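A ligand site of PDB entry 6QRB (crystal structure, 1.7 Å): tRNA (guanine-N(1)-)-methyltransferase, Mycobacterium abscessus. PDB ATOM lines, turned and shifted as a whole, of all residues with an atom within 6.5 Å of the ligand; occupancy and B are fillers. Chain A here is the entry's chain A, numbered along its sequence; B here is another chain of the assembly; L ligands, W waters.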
ATOM      1  N   VAL A  84      -4.873  22.744  -9.838  1.00  0.00           N
ATOM      2  CA  VAL A  84      -3.469  22.355  -9.951  1.00  0.00           C
ATOM      3  C   VAL A  84      -2.664  23.493 -10.583  1.00  0.00           C
ATOM      4  O   VAL A  84      -2.689  23.657 -11.801  1.00  0.00           O
ATOM      5  CB  VAL A  84      -3.273  21.076 -10.786  1.00  0.00           C
ATOM      6  CG1 VAL A  84      -1.804  20.621 -10.740  1.00  0.00           C
ATOM      7  CG2 VAL A  84      -4.221  19.965 -10.304  1.00  0.00           C
ATOM      8  N   PRO A  85      -1.969  24.293  -9.752  1.00  0.00           N
ATOM      9  CA  PRO A  85      -1.115  25.313 -10.351  1.00  0.00           C
ATOM     10  C   PRO A  85      -0.021  24.689 -11.199  1.00  0.00           C
ATOM     11  O   PRO A  85       0.564  23.685 -10.810  1.00  0.00           O
ATOM     12  CB  PRO A  85      -0.511  26.038  -9.137  1.00  0.00           C
ATOM     13  CG  PRO A  85      -1.533  25.857  -8.064  1.00  0.00           C
ATOM     14  CD  PRO A  85      -2.052  24.433  -8.290  1.00  0.00           C
ATOM     15  N   THR A  86       0.250  25.284 -12.348  1.00  0.00           N
ATOM     16  CA  THR A  86       1.302  24.819 -13.225  1.00  0.00           C
ATOM     17  C   THR A  86       1.579  25.918 -14.239  1.00  0.00           C
ATOM     18  O   THR A  86       0.665  26.603 -14.686  1.00  0.00           O
ATOM     19  CB  THR A  86       0.921  23.497 -13.964  1.00  0.00           C
ATOM     20  OG1 THR A  86       1.801  23.278 -15.071  1.00  0.00           O
ATOM     21  CG2 THR A  86      -0.508  23.526 -14.477  1.00  0.00           C
ATOM     22  N   PRO A  87       2.855  26.107 -14.591  1.00  0.00           N
ATOM     23  CA  PRO A  87       3.122  27.136 -15.611  1.00  0.00           C
ATOM     24  C   PRO A  87       2.630  26.690 -17.001  1.00  0.00           C
ATOM     25  O   PRO A  87       2.649  27.504 -17.920  1.00  0.00           O
ATOM     26  CB  PRO A  87       4.647  27.283 -15.567  1.00  0.00           C
ATOM     27  CG  PRO A  87       5.140  25.974 -15.059  1.00  0.00           C
ATOM     28  CD  PRO A  87       4.077  25.458 -14.107  1.00  0.00           C
ATOM     29  N   ALA A  88       2.181  25.448 -17.135  1.00  0.00           N
ATOM     30  CA  ALA A  88       1.613  24.981 -18.399  1.00  0.00           C
ATOM     31  C   ALA A  88       0.097  25.012 -18.359  1.00  0.00           C
ATOM     32  O   ALA A  88      -0.567  24.401 -19.194  1.00  0.00           O
ATOM     33  CB  ALA A  88       2.111  23.562 -18.719  1.00  0.00           C
ATOM     34  N   CYS A 110      -0.348  21.643  -4.654  1.00  0.00           N
ATOM     35  CA  CYS A 110       0.880  22.413  -4.921  1.00  0.00           C
ATOM     36  C   CYS A 110       2.053  21.525  -5.244  1.00  0.00           C
ATOM     37  O   CYS A 110       2.541  20.777  -4.399  1.00  0.00           O
ATOM     38  CB  CYS A 110       1.246  23.290  -3.723  1.00  0.00           C
ATOM     39  SG  CYS A 110      -0.006  24.506  -3.309  1.00  0.00           S
ATOM     40  N   GLY A 111       2.542  21.648  -6.472  1.00  0.00           N
ATOM     41  CA  GLY A 111       3.705  20.898  -6.886  1.00  0.00           C
ATOM     42  C   GLY A 111       5.013  21.591  -6.551  1.00  0.00           C
ATOM     43  O   GLY A 111       5.059  22.784  -6.229  1.00  0.00           O
ATOM     44  N   ARG A 112       6.076  20.799  -6.636  1.00  0.00           N
ATOM     45  CA  ARG A 112       7.454  21.265  -6.544  1.00  0.00           C
ATOM     46  C   ARG A 112       8.269  20.446  -7.557  1.00  0.00           C
ATOM     47  O   ARG A 112       7.699  19.649  -8.317  1.00  0.00           O
ATOM     48  CB  ARG A 112       7.996  21.098  -5.119  1.00  0.00           C
ATOM     49  CG  ARG A 112       7.523  22.179  -4.157  1.00  0.00           C
ATOM     50  CD  ARG A 112       8.509  23.335  -4.140  1.00  0.00           C
ATOM     51  NE  ARG A 112       7.871  24.552  -3.657  1.00  0.00           N
ATOM     52  CZ  ARG A 112       8.531  25.671  -3.386  1.00  0.00           C
ATOM     53  NH1 ARG A 112       9.856  25.720  -3.528  1.00  0.00           N
ATOM     54  NH2 ARG A 112       7.863  26.733  -2.953  1.00  0.00           N
ATOM     55  N   TYR A 113       9.585  20.650  -7.568  1.00  0.00           N
ATOM     56  CA  TYR A 113      10.463  19.951  -8.503  1.00  0.00           C
ATOM     57  C   TYR A 113       9.979  20.231  -9.935  1.00  0.00           C
ATOM     58  O   TYR A 113       9.709  21.385 -10.279  1.00  0.00           O
ATOM     59  CB  TYR A 113      10.489  18.444  -8.217  1.00  0.00           C
ATOM     60  CG  TYR A 113      10.856  18.067  -6.790  1.00  0.00           C
ATOM     61  CD1 TYR A 113      12.191  17.857  -6.435  1.00  0.00           C
ATOM     62  CD2 TYR A 113       9.886  17.894  -5.818  1.00  0.00           C
ATOM     63  CE1 TYR A 113      12.534  17.509  -5.137  1.00  0.00           C
ATOM     64  CE2 TYR A 113      10.220  17.547  -4.521  1.00  0.00           C
ATOM     65  CZ  TYR A 113      11.551  17.361  -4.187  1.00  0.00           C
ATOM     66  OH  TYR A 113      11.904  17.005  -2.895  1.00  0.00           O
ATOM     67  N   GLU A 114       9.868  19.200 -10.773  1.00  0.00           N
ATOM     68  CA  GLU A 114       9.377  19.410 -12.133  1.00  0.00           C
ATOM     69  C   GLU A 114       7.897  19.113 -12.260  1.00  0.00           C
ATOM     70  O   GLU A 114       7.393  18.843 -13.340  1.00  0.00           O
ATOM     71  CB  GLU A 114      10.183  18.554 -13.114  1.00  0.00           C
ATOM     72  CG  GLU A 114      11.661  18.857 -13.057  1.00  0.00           C
ATOM     73  CD  GLU A 114      11.982  20.262 -13.518  1.00  0.00           C
ATOM     74  OE1 GLU A 114      12.428  21.093 -12.692  1.00  0.00           O
ATOM     75  OE2 GLU A 114      11.768  20.538 -14.707  1.00  0.00           O
ATOM     76  N   GLY A 115       7.191  19.160 -11.130  1.00  0.00           N
ATOM     77  CA  GLY A 115       5.750  18.972 -11.168  1.00  0.00           C
ATOM     78  C   GLY A 115       5.296  17.566 -10.793  1.00  0.00           C
ATOM     79  O   GLY A 115       6.087  16.736 -10.363  1.00  0.00           O
ATOM     80  N   ILE A 116       4.003  17.324 -10.975  1.00  0.00           N
ATOM     81  CA  ILE A 116       3.368  16.080 -10.574  1.00  0.00           C
ATOM     82  C   ILE A 116       3.139  15.169 -11.773  1.00  0.00           C
ATOM     83  O   ILE A 116       2.706  15.617 -12.825  1.00  0.00           O
ATOM     84  CB  ILE A 116       2.013  16.383  -9.876  1.00  0.00           C
ATOM     85  CG1 ILE A 116       2.219  17.413  -8.764  1.00  0.00           C
ATOM     86  CG2 ILE A 116       1.342  15.113  -9.360  1.00  0.00           C
ATOM     87  CD1 ILE A 116       0.921  17.861  -8.100  1.00  0.00           C
ATOM     88  N   VAL A 133      -4.053  25.424 -13.957  1.00  0.00           N
ATOM     89  CA  VAL A 133      -4.042  26.865 -14.215  1.00  0.00           C
ATOM     90  C   VAL A 133      -2.701  27.509 -13.879  1.00  0.00           C
ATOM     91  O   VAL A 133      -1.979  27.033 -13.011  1.00  0.00           O
ATOM     92  CB  VAL A 133      -5.143  27.609 -13.416  1.00  0.00           C
ATOM     93  CG1 VAL A 133      -6.535  27.160 -13.851  1.00  0.00           C
ATOM     94  CG2 VAL A 133      -4.949  27.422 -11.896  1.00  0.00           C
ATOM     95  N   SER A 134      -2.395  28.619 -14.561  1.00  0.00           N
ATOM     96  CA  SER A 134      -1.196  29.419 -14.288  1.00  0.00           C
ATOM     97  C   SER A 134      -1.554  30.855 -13.909  1.00  0.00           C
ATOM     98  O   SER A 134      -2.438  31.429 -14.539  1.00  0.00           O
ATOM     99  CB  SER A 134      -0.284  29.457 -15.510  1.00  0.00           C
ATOM    100  OG  SER A 134       0.747  30.420 -15.330  1.00  0.00           O
ATOM    101  N   ILE A 135      -0.866  31.450 -12.929  1.00  0.00           N
ATOM    102  CA  ILE A 135      -1.214  32.794 -12.499  1.00  0.00           C
ATOM    103  C   ILE A 135      -0.475  33.875 -13.277  1.00  0.00           C
ATOM    104  O   ILE A 135      -0.711  35.064 -13.087  1.00  0.00           O
ATOM    105  CB  ILE A 135      -0.970  33.026 -11.008  1.00  0.00           C
ATOM    106  CG1 ILE A 135       0.501  32.786 -10.633  1.00  0.00           C
ATOM    107  CG2 ILE A 135      -1.916  32.144 -10.182  1.00  0.00           C
ATOM    108  CD1 ILE A 135       0.896  33.476  -9.316  1.00  0.00           C
ATOM    109  N   GLY A 136       0.416  33.472 -14.176  1.00  0.00           N
ATOM    110  CA  GLY A 136       1.133  34.485 -14.947  1.00  0.00           C
ATOM    111  C   GLY A 136       2.315  33.948 -15.715  1.00  0.00           C
ATOM    112  O   GLY A 136       2.742  32.803 -15.503  1.00  0.00           O
ATOM    113  N   ASP A 137       2.880  34.783 -16.579  1.00  0.00           N
ATOM    114  CA  ASP A 137       3.932  34.318 -17.457  1.00  0.00           C
ATOM    115  C   ASP A 137       5.339  34.554 -16.907  1.00  0.00           C
ATOM    116  O   ASP A 137       6.126  35.296 -17.489  1.00  0.00           O
ATOM    117  CB  ASP A 137       3.797  34.971 -18.825  1.00  0.00           C
ATOM    118  CG  ASP A 137       2.637  34.403 -19.627  1.00  0.00           C
ATOM    119  OD1 ASP A 137       2.253  33.241 -19.371  1.00  0.00           O
ATOM    120  OD2 ASP A 137       2.125  35.088 -20.536  1.00  0.00           O
ATOM    121  N   TYR A 138       5.633  33.912 -15.777  1.00  0.00           N
ATOM    122  CA  TYR A 138       6.925  33.941 -15.125  1.00  0.00           C
ATOM    123  C   TYR A 138       7.048  32.575 -14.462  1.00  0.00           C
ATOM    124  O   TYR A 138       6.028  31.878 -14.331  1.00  0.00           O
ATOM    125  CB  TYR A 138       7.020  35.065 -14.075  1.00  0.00           C
ATOM    126  CG  TYR A 138       5.688  35.309 -13.394  1.00  0.00           C
ATOM    127  CD1 TYR A 138       5.218  34.456 -12.399  1.00  0.00           C
ATOM    128  CD2 TYR A 138       4.880  36.376 -13.789  1.00  0.00           C
ATOM    129  CE1 TYR A 138       3.979  34.657 -11.802  1.00  0.00           C
ATOM    130  CE2 TYR A 138       3.633  36.599 -13.185  1.00  0.00           C
ATOM    131  CZ  TYR A 138       3.193  35.728 -12.202  1.00  0.00           C
ATOM    132  OH  TYR A 138       1.965  35.928 -11.619  1.00  0.00           O
ATOM    133  N   VAL A 139       8.253  32.222 -14.046  1.00  0.00           N
ATOM    134  CA  VAL A 139       8.534  30.935 -13.418  1.00  0.00           C
ATOM    135  C   VAL A 139       8.738  31.050 -11.918  1.00  0.00           C
ATOM    136  O   VAL A 139       9.550  31.848 -11.446  1.00  0.00           O
ATOM    137  CB  VAL A 139       9.776  30.284 -14.051  1.00  0.00           C
ATOM    138  CG1 VAL A 139      10.074  28.934 -13.383  1.00  0.00           C
ATOM    139  CG2 VAL A 139       9.585  30.125 -15.552  1.00  0.00           C
ATOM    140  N   LEU A 140       7.958  30.277 -11.152  1.00  0.00           N
ATOM    141  CA  LEU A 140       8.086  30.206  -9.702  1.00  0.00           C
ATOM    142  C   LEU A 140       8.816  28.920  -9.288  1.00  0.00           C
ATOM    143  O   LEU A 140       9.148  28.096 -10.148  1.00  0.00           O
ATOM    144  CB  LEU A 140       6.698  30.262  -9.068  1.00  0.00           C
ATOM    145  CG  LEU A 140       5.845  31.493  -9.457  1.00  0.00           C
ATOM    146  CD1 LEU A 140       4.383  31.281  -9.014  1.00  0.00           C
ATOM    147  CD2 LEU A 140       6.402  32.763  -8.838  1.00  0.00           C
ATOM    148  N   ASN A 141       9.051  28.724  -7.984  1.00  0.00           N
ATOM    149  CA  ASN A 141       9.702  27.500  -7.489  1.00  0.00           C
ATOM    150  C   ASN A 141       8.742  26.329  -7.283  1.00  0.00           C
ATOM    151  O   ASN A 141       9.173  25.174  -7.128  1.00  0.00           O
ATOM    152  CB  ASN A 141      10.418  27.782  -6.164  1.00  0.00           C
ATOM    153  CG  ASN A 141      11.669  28.621  -6.346  1.00  0.00           C
ATOM    154  OD1 ASN A 141      12.372  28.507  -7.352  1.00  0.00           O
ATOM    155  ND2 ASN A 141      11.943  29.481  -5.380  1.00  0.00           N
ATOM    156  N   GLY A 142       7.455  26.623  -7.278  1.00  0.00           N
ATOM    157  CA  GLY A 142       6.459  25.607  -6.980  1.00  0.00           C
ATOM    158  C   GLY A 142       5.092  26.241  -6.946  1.00  0.00           C
ATOM    159  O   GLY A 142       4.936  27.425  -7.268  1.00  0.00           O
ATOM    160  N   GLY A 143       4.075  25.478  -6.547  1.00  0.00           N
ATOM    161  CA  GLY A 143       2.706  25.945  -6.660  1.00  0.00           C
ATOM    162  C   GLY A 143       2.225  26.794  -5.487  1.00  0.00           C
ATOM    163  O   GLY A 143       1.132  27.360  -5.563  1.00  0.00           O
ATOM    164  N   GLU A 144       3.028  26.884  -4.422  1.00  0.00           N
ATOM    165  CA  GLU A 144       2.559  27.525  -3.189  1.00  0.00           C
ATOM    166  C   GLU A 144       2.255  29.027  -3.356  1.00  0.00           C
ATOM    167  O   GLU A 144       1.245  29.511  -2.865  1.00  0.00           O
ATOM    168  CB  GLU A 144       3.572  27.312  -2.057  1.00  0.00           C
ATOM    169  CG  GLU A 144       3.664  25.868  -1.525  1.00  0.00           C
ATOM    170  CD  GLU A 144       4.519  24.930  -2.399  1.00  0.00           C
ATOM    171  OE1 GLU A 144       5.205  25.400  -3.325  1.00  0.00           O
ATOM    172  OE2 GLU A 144       4.499  23.698  -2.136  1.00  0.00           O
ATOM    173  N   ALA A 146       1.422  30.517  -6.072  1.00  0.00           N
ATOM    174  CA  ALA A 146       0.240  30.558  -6.906  1.00  0.00           C
ATOM    175  C   ALA A 146      -0.999  30.265  -6.072  1.00  0.00           C
ATOM    176  O   ALA A 146      -2.030  30.889  -6.266  1.00  0.00           O
ATOM    177  CB  ALA A 146       0.359  29.548  -8.074  1.00  0.00           C
ATOM    178  N   ILE A 150      -4.320  32.600  -5.776  1.00  0.00           N
ATOM    179  CA  ILE A 150      -5.617  32.061  -6.178  1.00  0.00           C
ATOM    180  C   ILE A 150      -6.604  32.168  -4.997  1.00  0.00           C
ATOM    181  O   ILE A 150      -7.738  32.611  -5.164  1.00  0.00           O
ATOM    182  CB  ILE A 150      -5.497  30.598  -6.656  1.00  0.00           C
ATOM    183  CG1 ILE A 150      -4.816  30.562  -8.031  1.00  0.00           C
ATOM    184  CG2 ILE A 150      -6.876  29.945  -6.733  1.00  0.00           C
ATOM    185  CD1 ILE A 150      -4.248  29.165  -8.398  1.00  0.00           C
ATOM    186  N   ARG B 156      15.171  33.592  -7.900  1.00  0.00           N
ATOM    187  CA  ARG B 156      15.667  32.337  -8.451  1.00  0.00           C
ATOM    188  C   ARG B 156      16.589  32.560  -9.674  1.00  0.00           C
ATOM    189  O   ARG B 156      17.308  31.646 -10.077  1.00  0.00           O
ATOM    190  CB  ARG B 156      14.503  31.393  -8.787  1.00  0.00           C
ATOM    191  CG  ARG B 156      13.544  31.870  -9.831  1.00  0.00           C
ATOM    192  CD  ARG B 156      12.324  30.940  -9.902  1.00  0.00           C
ATOM    193  NE  ARG B 156      12.703  29.579 -10.266  1.00  0.00           N
ATOM    194  CZ  ARG B 156      13.061  29.205 -11.485  1.00  0.00           C
ATOM    195  NH1 ARG B 156      13.109  30.100 -12.474  1.00  0.00           N
ATOM    196  NH2 ARG B 156      13.382  27.942 -11.721  1.00  0.00           N
ATOM    197  N   GLU B 182       5.222  23.532 -21.185  1.00  0.00           N
ATOM    198  CA  GLU B 182       5.788  22.223 -20.890  1.00  0.00           C
ATOM    199  C   GLU B 182       4.766  21.122 -21.071  1.00  0.00           C
ATOM    200  O   GLU B 182       3.595  21.282 -20.705  1.00  0.00           O
ATOM    201  CB  GLU B 182       6.338  22.169 -19.456  1.00  0.00           C
ATOM    202  CG  GLU B 182       7.578  23.016 -19.211  1.00  0.00           C
ATOM    203  CD  GLU B 182       7.251  24.475 -18.906  1.00  0.00           C
ATOM    204  OE1 GLU B 182       6.061  24.864 -19.011  1.00  0.00           O
ATOM    205  OE2 GLU B 182       8.187  25.214 -18.545  1.00  0.00           O
ATOM    206  N   GLY B 183       5.202  20.005 -21.619  1.00  0.00           N
ATOM    207  CA  GLY B 183       4.351  18.841 -21.779  1.00  0.00           C
ATOM    208  C   GLY B 183       4.311  18.075 -20.466  1.00  0.00           C
ATOM    209  O   GLY B 183       4.872  18.516 -19.468  1.00  0.00           O
ATOM    210  N   SER B 185       4.845  15.079 -17.559  1.00  0.00           N
ATOM    211  CA  SER B 185       5.973  14.312 -17.036  1.00  0.00           C
ATOM    212  C   SER B 185       5.469  13.090 -16.291  1.00  0.00           C
ATOM    213  O   SER B 185       4.362  13.113 -15.771  1.00  0.00           O
ATOM    214  CB  SER B 185       6.829  15.165 -16.099  1.00  0.00           C
ATOM    215  OG  SER B 185       7.501  16.193 -16.803  1.00  0.00           O
ATOM    216  N   ARG B 220      -0.516  21.266 -26.319  1.00  0.00           N
ATOM    217  CA  ARG B 220      -0.898  21.937 -25.089  1.00  0.00           C
ATOM    218  C   ARG B 220      -0.945  23.451 -25.262  1.00  0.00           C
ATOM    219  O   ARG B 220      -1.835  24.124 -24.752  1.00  0.00           O
ATOM    220  CB  ARG B 220       0.083  21.580 -23.978  1.00  0.00           C
ATOM    221  CG  ARG B 220      -0.419  21.912 -22.599  1.00  0.00           C
ATOM    222  CD  ARG B 220       0.492  21.321 -21.561  1.00  0.00           C
ATOM    223  NE  ARG B 220       0.004  20.033 -21.075  1.00  0.00           N
ATOM    224  CZ  ARG B 220       0.550  19.376 -20.061  1.00  0.00           C
ATOM    225  NH1 ARG B 220       1.606  19.882 -19.439  1.00  0.00           N
ATOM    226  NH2 ARG B 220       0.049  18.205 -19.661  1.00  0.00           N
HETATM  227  C1  LIG L   1       3.722  24.734 -10.096  1.00  0.00           C
HETATM  228  C2  LIG L   1       7.057  23.172  -9.710  1.00  0.00           C
HETATM  229  C3  LIG L   1       8.664  24.853 -10.480  1.00  0.00           C
HETATM  230  C4  LIG L   1       8.514  24.965 -12.963  1.00  0.00           C
HETATM  231  C5  LIG L   1       7.568  22.738 -14.475  1.00  0.00           C
HETATM  232  C6  LIG L   1       6.833  22.223 -13.351  1.00  0.00           C
HETATM  233  C7  LIG L   1       5.507  21.776 -13.514  1.00  0.00           C
HETATM  234  C8  LIG L   1       5.607  22.275 -15.851  1.00  0.00           C
HETATM  235  C9  LIG L   1      10.433  24.989 -14.303  1.00  0.00           C
HETATM  236  C10 LIG L   1      10.655  24.986 -11.861  1.00  0.00           C
HETATM  237  N1  LIG L   1       2.723  31.094 -13.161  1.00  0.00           N
HETATM  238  C11 LIG L   1       3.613  30.092 -12.667  1.00  0.00           C
HETATM  239  N2  LIG L   1       4.893  30.073 -12.776  1.00  0.00           N
HETATM  240  N3  LIG L   1       5.368  28.876 -12.113  1.00  0.00           N
HETATM  241  C12 LIG L   1       4.391  28.228 -11.616  1.00  0.00           C
HETATM  242  C13 LIG L   1       4.609  26.871 -10.978  1.00  0.00           C
HETATM  243  C14 LIG L   1       5.902  26.398 -10.924  1.00  0.00           C
HETATM  244  C15 LIG L   1       6.156  25.061 -10.409  1.00  0.00           C
HETATM  245  C16 LIG L   1       5.050  24.252  -9.995  1.00  0.00           C
HETATM  246  C17 LIG L   1       3.457  26.014 -10.587  1.00  0.00           C
HETATM  247  C18 LIG L   1       5.610  23.056  -9.572  1.00  0.00           C
HETATM  248  N4  LIG L   1       7.328  24.352 -10.227  1.00  0.00           N
HETATM  249  C19 LIG L   1       9.322  24.443 -11.811  1.00  0.00           C
HETATM  250  N5  LIG L   1       9.087  24.530 -14.191  1.00  0.00           N
HETATM  251  C20 LIG L   1       9.026  23.250 -14.306  1.00  0.00           C
HETATM  252  C21 LIG L   1       4.903  21.795 -14.771  1.00  0.00           C
HETATM  253  C22 LIG L   1       6.989  22.755 -15.679  1.00  0.00           C
HETATM  254  C23 LIG L   1      11.286  24.664 -13.082  1.00  0.00           C
HETATM  255  C24 LIG L   1       3.201  28.910 -11.959  1.00  0.00           C
HETATM  256  C25 LIG L   1       1.795  28.638 -11.663  1.00  0.00           C
HETATM  257  N6  LIG L   1       0.626  28.511 -11.473  1.00  0.00           N
HETATM  258  O   HOH W   1       1.791  20.905 -16.004  1.00  0.00           O
HETATM  259  O   HOH W   2       8.539  26.401 -16.414  1.00  0.00           O
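N2 of the ligand is in hydrogen-bond range of O of Tyr 138 (2.6 Å).
O of Gly 136 is in hydrogen-bond range of N1 of the ligand (2.9 Å).
The side-chain hydroxyl (OG) of Ser 134 is in hydrogen-bond range of a nitrogen (N1) of the ligand, at 3.0 Å.
The backbone NH of Leu 140 lies within hydrogen-bond range of a nitrogen (N3) of the ligand (3.1 Å).
N of Thr 86 is in hydrogen-bond range of N6 of the ligand.
OH of Tyr 138 lies within hydrogen-bond range of O of Ile 135 (3.2 Å).
OG of Ser 134 lies within hydrogen-bond range of O of Gly 136, at 3.1 Å.
The backbone NH (N) of Thr 86 is in hydrogen-bond range of the backbone carbonyl oxygen (O) of Val 133 (2.9 Å).
The side-chain hydroxyl of Thr 86 sits close to the backbone NH of Ala 88 (3.0 Å).
N of Val 133 lies within hydrogen-bond range of O of Val 84, 3.1 Å away.
The backbone carbonyl oxygen (O) of Gly 111 is in hydrogen-bond range of the backbone NH (N) of Gly 143 (2.9 Å).
The side-chain amide oxygen (OD1) of Asn 141 is in hydrogen-bond range of the guanidinium group (NE) of Arg 156 of chain B.
NE of Arg 112 lies within salt-bridge range of OE1 of Glu 144, 2.8 Å away.
A nitrogen (N6) of the ligand lies close to the backbone carbonyl oxygen (O) of Val 133 (3.4 Å).
Merely in contact with the ligand: Pro 85 (3.4 Å), Pro 87 (3.5 Å), Gly 111 (3.4 Å), Arg 112 (3.7 Å), Tyr 113 (3.2 Å), Glu 114 (3.4 Å), Gly 115 (3.7 Å), Ile 135 (3.6 Å), Val 139 (3.8 Å), Asn 141 (3.4 Å), Gly 142 (3.5 Å), Gly 143 (3.6 Å), Ala 146 (3.6 Å) and Glu 182 of chain B (3.6 Å).
Hydrophobic or aromatic side chains within 4 Å of the ligand: Pro 85, Pro 87, Ile 135, Leu 140 and Ala 146.
Of the 31 residues printed, 20 come within 4 Å of the ligand.
Along chain A the residues within 4 Å of the ligand span positions 85 to 146.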
